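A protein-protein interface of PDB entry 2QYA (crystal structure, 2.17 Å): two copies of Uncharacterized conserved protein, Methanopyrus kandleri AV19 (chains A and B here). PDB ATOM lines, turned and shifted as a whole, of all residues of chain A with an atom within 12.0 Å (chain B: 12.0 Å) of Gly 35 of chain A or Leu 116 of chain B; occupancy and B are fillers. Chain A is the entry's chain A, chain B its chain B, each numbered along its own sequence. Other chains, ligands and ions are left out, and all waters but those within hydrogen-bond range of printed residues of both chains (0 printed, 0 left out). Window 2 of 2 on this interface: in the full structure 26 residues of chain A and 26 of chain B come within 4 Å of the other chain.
Of the 9 printed residues of chain B, 4 touch a printed residue of chain A. Printed residues of chain B that touch a printed residue of chain A: Asp 68, Glu 69, Pro 114 and Leu 116. Hydrophobic or aromatic side chains of chain B that line the printed part of chain A: Pro 114 and Leu 116. Among the printed residues, 9 pairs touch across the chains. Among the printed residues, no Asp or Glu carboxylate lies within 4 Å of a Lys or Arg side-chain nitrogen of the other chain.
No position is printed for both chains.
The backbone carbonyl oxygen (O) of Asp 68 of chain B lies within hydrogen-bond range of the guanidinium group (NH2) of Arg 36 of chain A.
Among the printed residues, pairs that only touch across the chains: Tyr 33 of chain A with Pro 114 of chain B (3.6 Å), Lys 34 of chain A with Pro 114 of chain B (3.9 Å), Lys 34 of chain A with Leu 116 of chain B (3.4 Å), Gly 35 of chain A with Leu 116 of chain B (3.8 Å), Arg 36 of chain A with Glu 69 of chain B (3.2 Å), Arg 36 of chain A with Pro 114 of chain B (3.6 Å), Leu 38 of chain A with Glu 69 of chain B (3.2 Å) and His 39 of chain A with Glu 69 of chain B (3.99 Å).
Of chain B, only Leu 116 comes within 4 Å of Gly 35 of chain A. Of chain A, only Lys 34 and Gly 35 come within 4 Å of Leu 116 of chain B. No residue of chain B comes within 4 Å of Lys 32 of chain A. Lys 34 of chain A touches two residues of chain B. Arg 36 of chain A touches just these residues of chain B: Asp 68, Glu 69 and Pro 114. No residue of chain B comes within 4 Å of Thr 37 of chain A. Pro 114 of chain B touches just these residues of chain A: Tyr 33 (3.6 Å), Lys 34 (3.9 Å) and Arg 36 (3.6 Å). No residue of chain A comes within 4 Å of Phe 115 of chain B. No residue of chain A comes within 4 Å of Glu 117 of chain B. Of the printed residues of chain B, Leu 38 of chain A touches Glu 69 (3.2 Å). Of the printed residues of chain B, Tyr 33 of chain A touches Pro 114 (3.6 Å). Printed residues of chain A within 4 Å of Asp 68 of chain B: Arg 36. Of the printed residues of chain A, Glu 69 of chain B touches Arg 36, Leu 38 and His 39. Of the printed residues of chain B, His 39 of chain A touches Glu 69 (3.99 Å). Glu 98 of chain A touches none of the printed residues of chain B. Glu 113 of chain B touches none of the printed residues of chain A. The nearest residue of chain B that does not touch Gly 35 of chain A is Pro 114 of chain B (5.8 Å). The nearest printed residue of chain B that does not touch Leu 38 of chain A is Asp 68 of chain B (8.4 Å).
The backbone NH of Leu 38 of chain A sits at hydrogen-bond distance from the backbone carbonyl oxygen of Leu 31 of chain A (2.7 Å).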
ATOM      1  N   GLU A  30     -16.898 -18.542 -17.312  1.00  0.00           N
ATOM      2  CA  GLU A  30     -16.713 -19.668 -16.401  1.00  0.00           C
ATOM      3  C   GLU A  30     -16.275 -20.916 -17.153  1.00  0.00           C
ATOM      4  O   GLU A  30     -16.855 -21.279 -18.178  1.00  0.00           O
ATOM      5  CB  GLU A  30     -17.972 -19.939 -15.573  1.00  0.00           C
ATOM      6  CG  GLU A  30     -18.182 -18.917 -14.461  1.00  0.00           C
ATOM      7  CD  GLU A  30     -19.174 -19.368 -13.391  1.00  0.00           C
ATOM      8  OE1 GLU A  30     -19.503 -20.584 -13.319  1.00  0.00           O
ATOM      9  OE2 GLU A  30     -19.618 -18.486 -12.613  1.00  0.00           O
ATOM     10  N   LEU A  31     -15.225 -21.549 -16.651  1.00  0.00           N
ATOM     11  CA  LEU A  31     -14.714 -22.752 -17.275  1.00  0.00           C
ATOM     12  C   LEU A  31     -14.870 -23.910 -16.316  1.00  0.00           C
ATOM     13  O   LEU A  31     -14.509 -23.818 -15.137  1.00  0.00           O
ATOM     14  CB  LEU A  31     -13.245 -22.596 -17.691  1.00  0.00           C
ATOM     15  CG  LEU A  31     -12.781 -21.355 -18.467  1.00  0.00           C
ATOM     16  CD1 LEU A  31     -11.278 -21.429 -18.662  1.00  0.00           C
ATOM     17  CD2 LEU A  31     -13.493 -21.226 -19.809  1.00  0.00           C
ATOM     18  N   LYS A  32     -15.418 -24.999 -16.837  1.00  0.00           N
ATOM     19  CA  LYS A  32     -15.626 -26.205 -16.062  1.00  0.00           C
ATOM     20  C   LYS A  32     -14.632 -27.258 -16.517  1.00  0.00           C
ATOM     21  O   LYS A  32     -14.444 -27.457 -17.715  1.00  0.00           O
ATOM     22  CB  LYS A  32     -17.067 -26.698 -16.228  1.00  0.00           C
ATOM     23  CG  LYS A  32     -18.049 -26.133 -15.199  1.00  0.00           C
ATOM     24  CD  LYS A  32     -19.499 -26.515 -15.530  1.00  0.00           C
ATOM     25  CE  LYS A  32     -20.363 -26.734 -14.275  1.00  0.00           C
ATOM     26  NZ  LYS A  32     -20.483 -25.515 -13.403  1.00  0.00           N
ATOM     27  N   TYR A  33     -13.971 -27.915 -15.569  1.00  0.00           N
ATOM     28  CA  TYR A  33     -13.092 -29.025 -15.920  1.00  0.00           C
ATOM     29  C   TYR A  33     -12.908 -30.018 -14.760  1.00  0.00           C
ATOM     30  O   TYR A  33     -12.554 -29.633 -13.639  1.00  0.00           O
ATOM     31  CB  TYR A  33     -11.755 -28.514 -16.504  1.00  0.00           C
ATOM     32  CG  TYR A  33     -10.648 -28.295 -15.497  1.00  0.00           C
ATOM     33  CD1 TYR A  33     -10.734 -27.286 -14.540  1.00  0.00           C
ATOM     34  CD2 TYR A  33      -9.510 -29.105 -15.508  1.00  0.00           C
ATOM     35  CE1 TYR A  33      -9.720 -27.099 -13.614  1.00  0.00           C
ATOM     36  CE2 TYR A  33      -8.491 -28.924 -14.587  1.00  0.00           C
ATOM     37  CZ  TYR A  33      -8.602 -27.924 -13.643  1.00  0.00           C
ATOM     38  OH  TYR A  33      -7.593 -27.745 -12.729  1.00  0.00           O
ATOM     39  N   LYS A  34     -13.178 -31.290 -15.059  1.00  0.00           N
ATOM     40  CA  LYS A  34     -13.190 -32.392 -14.078  1.00  0.00           C
ATOM     41  C   LYS A  34     -13.850 -32.042 -12.734  1.00  0.00           C
ATOM     42  O   LYS A  34     -13.292 -32.305 -11.664  1.00  0.00           O
ATOM     43  CB  LYS A  34     -11.786 -32.988 -13.887  1.00  0.00           C
ATOM     44  CG  LYS A  34     -11.353 -33.938 -15.008  1.00  0.00           C
ATOM     45  CD  LYS A  34     -10.597 -35.167 -14.459  1.00  0.00           C
ATOM     46  CE  LYS A  34      -9.747 -35.849 -15.545  1.00  0.00           C
ATOM     47  NZ  LYS A  34      -9.118 -37.164 -15.129  1.00  0.00           N
ATOM     48  N   GLY A  35     -15.043 -31.451 -12.806  1.00  0.00           N
ATOM     49  CA  GLY A  35     -15.822 -31.109 -11.616  1.00  0.00           C
ATOM     50  C   GLY A  35     -15.515 -29.749 -11.021  1.00  0.00           C
ATOM     51  O   GLY A  35     -16.185 -29.316 -10.079  1.00  0.00           O
ATOM     52  N   ARG A  36     -14.498 -29.078 -11.562  1.00  0.00           N
ATOM     53  CA  ARG A  36     -14.115 -27.742 -11.103  1.00  0.00           C
ATOM     54  C   ARG A  36     -14.888 -26.627 -11.801  1.00  0.00           C
ATOM     55  O   ARG A  36     -15.524 -26.833 -12.836  1.00  0.00           O
ATOM     56  CB  ARG A  36     -12.609 -27.497 -11.279  1.00  0.00           C
ATOM     57  CG  ARG A  36     -11.758 -27.995 -10.130  1.00  0.00           C
ATOM     58  CD  ARG A  36     -10.368 -27.316 -10.093  1.00  0.00           C
ATOM     59  NE  ARG A  36     -10.346 -26.080  -9.302  1.00  0.00           N
ATOM     60  CZ  ARG A  36     -10.535 -26.011  -7.981  1.00  0.00           C
ATOM     61  NH1 ARG A  36     -10.785 -27.100  -7.259  1.00  0.00           N
ATOM     62  NH2 ARG A  36     -10.487 -24.833  -7.376  1.00  0.00           N
ATOM     63  N   THR A  37     -14.827 -25.444 -11.200  1.00  0.00           N
ATOM     64  CA  THR A  37     -15.375 -24.227 -11.796  1.00  0.00           C
ATOM     65  C   THR A  37     -14.301 -23.174 -11.671  1.00  0.00           C
ATOM     66  O   THR A  37     -13.925 -22.788 -10.559  1.00  0.00           O
ATOM     67  CB  THR A  37     -16.624 -23.712 -11.053  1.00  0.00           C
ATOM     68  OG1 THR A  37     -17.268 -24.793 -10.365  1.00  0.00           O
ATOM     69  CG2 THR A  37     -17.594 -23.045 -12.026  1.00  0.00           C
ATOM     70  N   LEU A  38     -13.778 -22.735 -12.806  1.00  0.00           N
ATOM     71  CA  LEU A  38     -12.896 -21.588 -12.805  1.00  0.00           C
ATOM     72  C   LEU A  38     -13.686 -20.352 -13.204  1.00  0.00           C
ATOM     73  O   LEU A  38     -14.320 -20.311 -14.254  1.00  0.00           O
ATOM     74  CB  LEU A  38     -11.662 -21.798 -13.705  1.00  0.00           C
ATOM     75  CG  LEU A  38     -10.672 -20.619 -13.823  1.00  0.00           C
ATOM     76  CD1 LEU A  38     -10.123 -20.126 -12.469  1.00  0.00           C
ATOM     77  CD2 LEU A  38      -9.525 -20.914 -14.792  1.00  0.00           C
ATOM     78  N   HIS A  39     -13.651 -19.361 -12.326  1.00  0.00           N
ATOM     79  CA  HIS A  39     -14.189 -18.033 -12.604  1.00  0.00           C
ATOM     80  C   HIS A  39     -13.050 -17.150 -13.111  1.00  0.00           C
ATOM     81  O   HIS A  39     -12.105 -16.871 -12.374  1.00  0.00           O
ATOM     82  CB  HIS A  39     -14.804 -17.440 -11.327  1.00  0.00           C
ATOM     83  CG  HIS A  39     -15.705 -18.389 -10.598  1.00  0.00           C
ATOM     84  ND1 HIS A  39     -15.269 -19.171  -9.550  1.00  0.00           N
ATOM     85  CD2 HIS A  39     -17.012 -18.697 -10.780  1.00  0.00           C
ATOM     86  CE1 HIS A  39     -16.272 -19.910  -9.109  1.00  0.00           C
ATOM     87  NE2 HIS A  39     -17.342 -19.640  -9.836  1.00  0.00           N
ATOM     88  N   GLU A  98      -3.493 -27.056 -20.949  1.00  0.00           N
ATOM     89  CA  GLU A  98      -4.847 -26.617 -21.193  1.00  0.00           C
ATOM     90  C   GLU A  98      -5.606 -26.705 -19.892  1.00  0.00           C
ATOM     91  O   GLU A  98      -5.244 -27.489 -19.010  1.00  0.00           O
ATOM     92  CB  GLU A  98      -5.541 -27.470 -22.269  1.00  0.00           C
ATOM     93  CG  GLU A  98      -6.204 -28.720 -21.720  1.00  0.00           C
ATOM     94  CD  GLU A  98      -7.625 -28.879 -22.223  1.00  0.00           C
ATOM     95  OE1 GLU A  98      -7.827 -28.768 -23.466  1.00  0.00           O
ATOM     96  OE2 GLU A  98      -8.525 -29.098 -21.369  1.00  0.00           O
ATOM     97  N   LEU A  99      -6.652 -25.899 -19.770  1.00  0.00           N
ATOM     98  CA  LEU A  99      -7.454 -25.867 -18.557  1.00  0.00           C
ATOM     99  C   LEU A  99      -8.901 -25.564 -18.900  1.00  0.00           C
ATOM    100  O   LEU A  99      -9.270 -24.406 -19.078  1.00  0.00           O
ATOM    101  CB  LEU A  99      -6.908 -24.810 -17.596  1.00  0.00           C
ATOM    102  CG  LEU A  99      -6.975 -25.160 -16.110  1.00  0.00           C
ATOM    103  CD1 LEU A  99      -6.043 -26.357 -15.775  1.00  0.00           C
ATOM    104  CD2 LEU A  99      -6.656 -23.916 -15.254  1.00  0.00           C
ATOM    105  N   GLY A 100      -9.715 -26.610 -19.002  1.00  0.00           N
ATOM    106  CA  GLY A 100     -11.118 -26.477 -19.388  1.00  0.00           C
ATOM    107  C   GLY A 100     -11.274 -26.334 -20.886  1.00  0.00           C
ATOM    108  O   GLY A 100     -12.057 -25.505 -21.351  1.00  0.00           O
ATOM    109  N   GLY A 101     -10.511 -27.125 -21.641  1.00  0.00           N
ATOM    110  CA  GLY A 101     -10.508 -27.035 -23.105  1.00  0.00           C
ATOM    111  C   GLY A 101      -9.837 -25.783 -23.647  1.00  0.00           C
ATOM    112  O   GLY A 101      -9.731 -25.613 -24.880  1.00  0.00           O
ATOM    113  N   ASP B  68      -7.004 -24.289  -2.946  1.00  0.00           N
ATOM    114  CA  ASP B  68      -7.621 -25.202  -3.894  1.00  0.00           C
ATOM    115  C   ASP B  68      -7.828 -24.604  -5.294  1.00  0.00           C
ATOM    116  O   ASP B  68      -7.920 -25.352  -6.272  1.00  0.00           O
ATOM    117  CB  ASP B  68      -8.932 -25.767  -3.322  1.00  0.00           C
ATOM    118  CG  ASP B  68      -8.732 -27.113  -2.598  1.00  0.00           C
ATOM    119  OD1 ASP B  68      -7.997 -27.163  -1.578  1.00  0.00           O
ATOM    120  OD2 ASP B  68      -9.311 -28.128  -3.051  1.00  0.00           O
ATOM    121  N   GLU B  69      -7.881 -23.271  -5.394  1.00  0.00           N
ATOM    122  CA  GLU B  69      -8.138 -22.593  -6.682  1.00  0.00           C
ATOM    123  C   GLU B  69      -6.888 -21.953  -7.253  1.00  0.00           C
ATOM    124  O   GLU B  69      -6.736 -21.896  -8.467  1.00  0.00           O
ATOM    125  CB  GLU B  69      -9.242 -21.531  -6.554  1.00  0.00           C
ATOM    126  CG  GLU B  69     -10.418 -21.650  -7.586  1.00  0.00           C
ATOM    127  CD  GLU B  69     -10.251 -20.805  -8.868  1.00  0.00           C
ATOM    128  OE1 GLU B  69     -11.213 -20.080  -9.249  1.00  0.00           O
ATOM    129  OE2 GLU B  69      -9.169 -20.877  -9.504  1.00  0.00           O
ATOM    130  N   ARG B 112      -3.063 -29.307  -6.942  1.00  0.00           N
ATOM    131  CA  ARG B 112      -3.260 -30.649  -7.471  1.00  0.00           C
ATOM    132  C   ARG B 112      -4.254 -30.678  -8.610  1.00  0.00           C
ATOM    133  O   ARG B 112      -5.189 -29.904  -8.624  1.00  0.00           O
ATOM    134  CB  ARG B 112      -3.823 -31.540  -6.366  1.00  0.00           C
ATOM    135  CG  ARG B 112      -2.987 -31.574  -5.116  1.00  0.00           C
ATOM    136  CD  ARG B 112      -1.820 -32.464  -5.356  1.00  0.00           C
ATOM    137  NE  ARG B 112      -0.584 -31.977  -4.757  1.00  0.00           N
ATOM    138  CZ  ARG B 112       0.465 -32.760  -4.524  1.00  0.00           C
ATOM    139  NH1 ARG B 112       1.555 -32.246  -3.975  1.00  0.00           N
ATOM    140  NH2 ARG B 112       0.417 -34.062  -4.839  1.00  0.00           N
ATOM    141  N   GLU B 113      -4.049 -31.587  -9.557  1.00  0.00           N
ATOM    142  CA  GLU B 113      -5.075 -31.974 -10.523  1.00  0.00           C
ATOM    143  C   GLU B 113      -6.407 -32.125  -9.752  1.00  0.00           C
ATOM    144  O   GLU B 113      -6.411 -32.486  -8.564  1.00  0.00           O
ATOM    145  CB  GLU B 113      -4.670 -33.313 -11.156  1.00  0.00           C
ATOM    146  CG  GLU B 113      -4.779 -33.431 -12.656  1.00  0.00           C
ATOM    147  CD  GLU B 113      -3.500 -33.042 -13.407  1.00  0.00           C
ATOM    148  OE1 GLU B 113      -2.398 -33.495 -13.042  1.00  0.00           O
ATOM    149  OE2 GLU B 113      -3.596 -32.294 -14.394  1.00  0.00           O
ATOM    150  N   PRO B 114      -7.552 -31.825 -10.391  1.00  0.00           N
ATOM    151  CA  PRO B 114      -8.768 -31.977  -9.571  1.00  0.00           C
ATOM    152  C   PRO B 114      -9.360 -33.402  -9.612  1.00  0.00           C
ATOM    153  O   PRO B 114      -9.236 -34.118 -10.605  1.00  0.00           O
ATOM    154  CB  PRO B 114      -9.730 -30.959 -10.183  1.00  0.00           C
ATOM    155  CG  PRO B 114      -9.338 -30.902 -11.656  1.00  0.00           C
ATOM    156  CD  PRO B 114      -7.861 -31.359 -11.760  1.00  0.00           C
ATOM    157  N   PHE B 115      -9.987 -33.783  -8.507  1.00  0.00           N
ATOM    158  CA  PHE B 115     -10.599 -35.090  -8.333  1.00  0.00           C
ATOM    159  C   PHE B 115     -12.120 -35.028  -8.655  1.00  0.00           C
ATOM    160  O   PHE B 115     -12.920 -34.609  -7.833  1.00  0.00           O
ATOM    161  CB  PHE B 115     -10.338 -35.544  -6.895  1.00  0.00           C
ATOM    162  CG  PHE B 115     -10.695 -36.971  -6.613  1.00  0.00           C
ATOM    163  CD1 PHE B 115     -10.692 -37.925  -7.613  1.00  0.00           C
ATOM    164  CD2 PHE B 115     -10.975 -37.371  -5.322  1.00  0.00           C
ATOM    165  CE1 PHE B 115     -10.996 -39.240  -7.315  1.00  0.00           C
ATOM    166  CE2 PHE B 115     -11.294 -38.675  -5.033  1.00  0.00           C
ATOM    167  CZ  PHE B 115     -11.303 -39.607  -6.023  1.00  0.00           C
ATOM    168  N   LEU B 116     -12.489 -35.452  -9.863  1.00  0.00           N
ATOM    169  CA  LEU B 116     -13.882 -35.414 -10.336  1.00  0.00           C
ATOM    170  C   LEU B 116     -14.875 -36.122  -9.404  1.00  0.00           C
ATOM    171  O   LEU B 116     -16.003 -35.648  -9.205  1.00  0.00           O
ATOM    172  CB  LEU B 116     -13.980 -36.007 -11.744  1.00  0.00           C
ATOM    173  CG  LEU B 116     -15.356 -36.328 -12.349  1.00  0.00           C
ATOM    174  CD1 LEU B 116     -16.216 -35.091 -12.510  1.00  0.00           C
ATOM    175  CD2 LEU B 116     -15.167 -37.047 -13.710  1.00  0.00           C
ATOM    176  N   GLU B 117     -14.462 -37.262  -8.851  1.00  0.00           N
ATOM    177  CA  GLU B 117     -15.279 -37.955  -7.880  1.00  0.00           C
ATOM    178  C   GLU B 117     -15.061 -37.361  -6.490  1.00  0.00           C
ATOM    179  O   GLU B 117     -15.431 -37.969  -5.503  1.00  0.00           O
ATOM    180  CB  GLU B 117     -14.975 -39.461  -7.910  1.00  0.00           C
ATOM    181  CG  GLU B 117     -15.424 -40.179  -9.192  1.00  0.00           C
ATOM    182  CD  GLU B 117     -14.374 -40.146 -10.312  1.00  0.00           C
ATOM    183  OE1 GLU B 117     -13.326 -39.460 -10.150  1.00  0.00           O
ATOM    184  OE2 GLU B 117     -14.601 -40.813 -11.358  1.00  0.00           O
ATOM    185  N   GLY B 118     -14.461 -36.168  -6.413  1.00  0.00           N
ATOM    186  CA  GLY B 118     -14.004 -35.602  -5.132  1.00  0.00           C
ATOM    187  C   GLY B 118     -14.980 -34.709  -4.388  1.00  0.00           C
ATOM    188  O   GLY B 118     -16.181 -34.800  -4.622  1.00  0.00           O
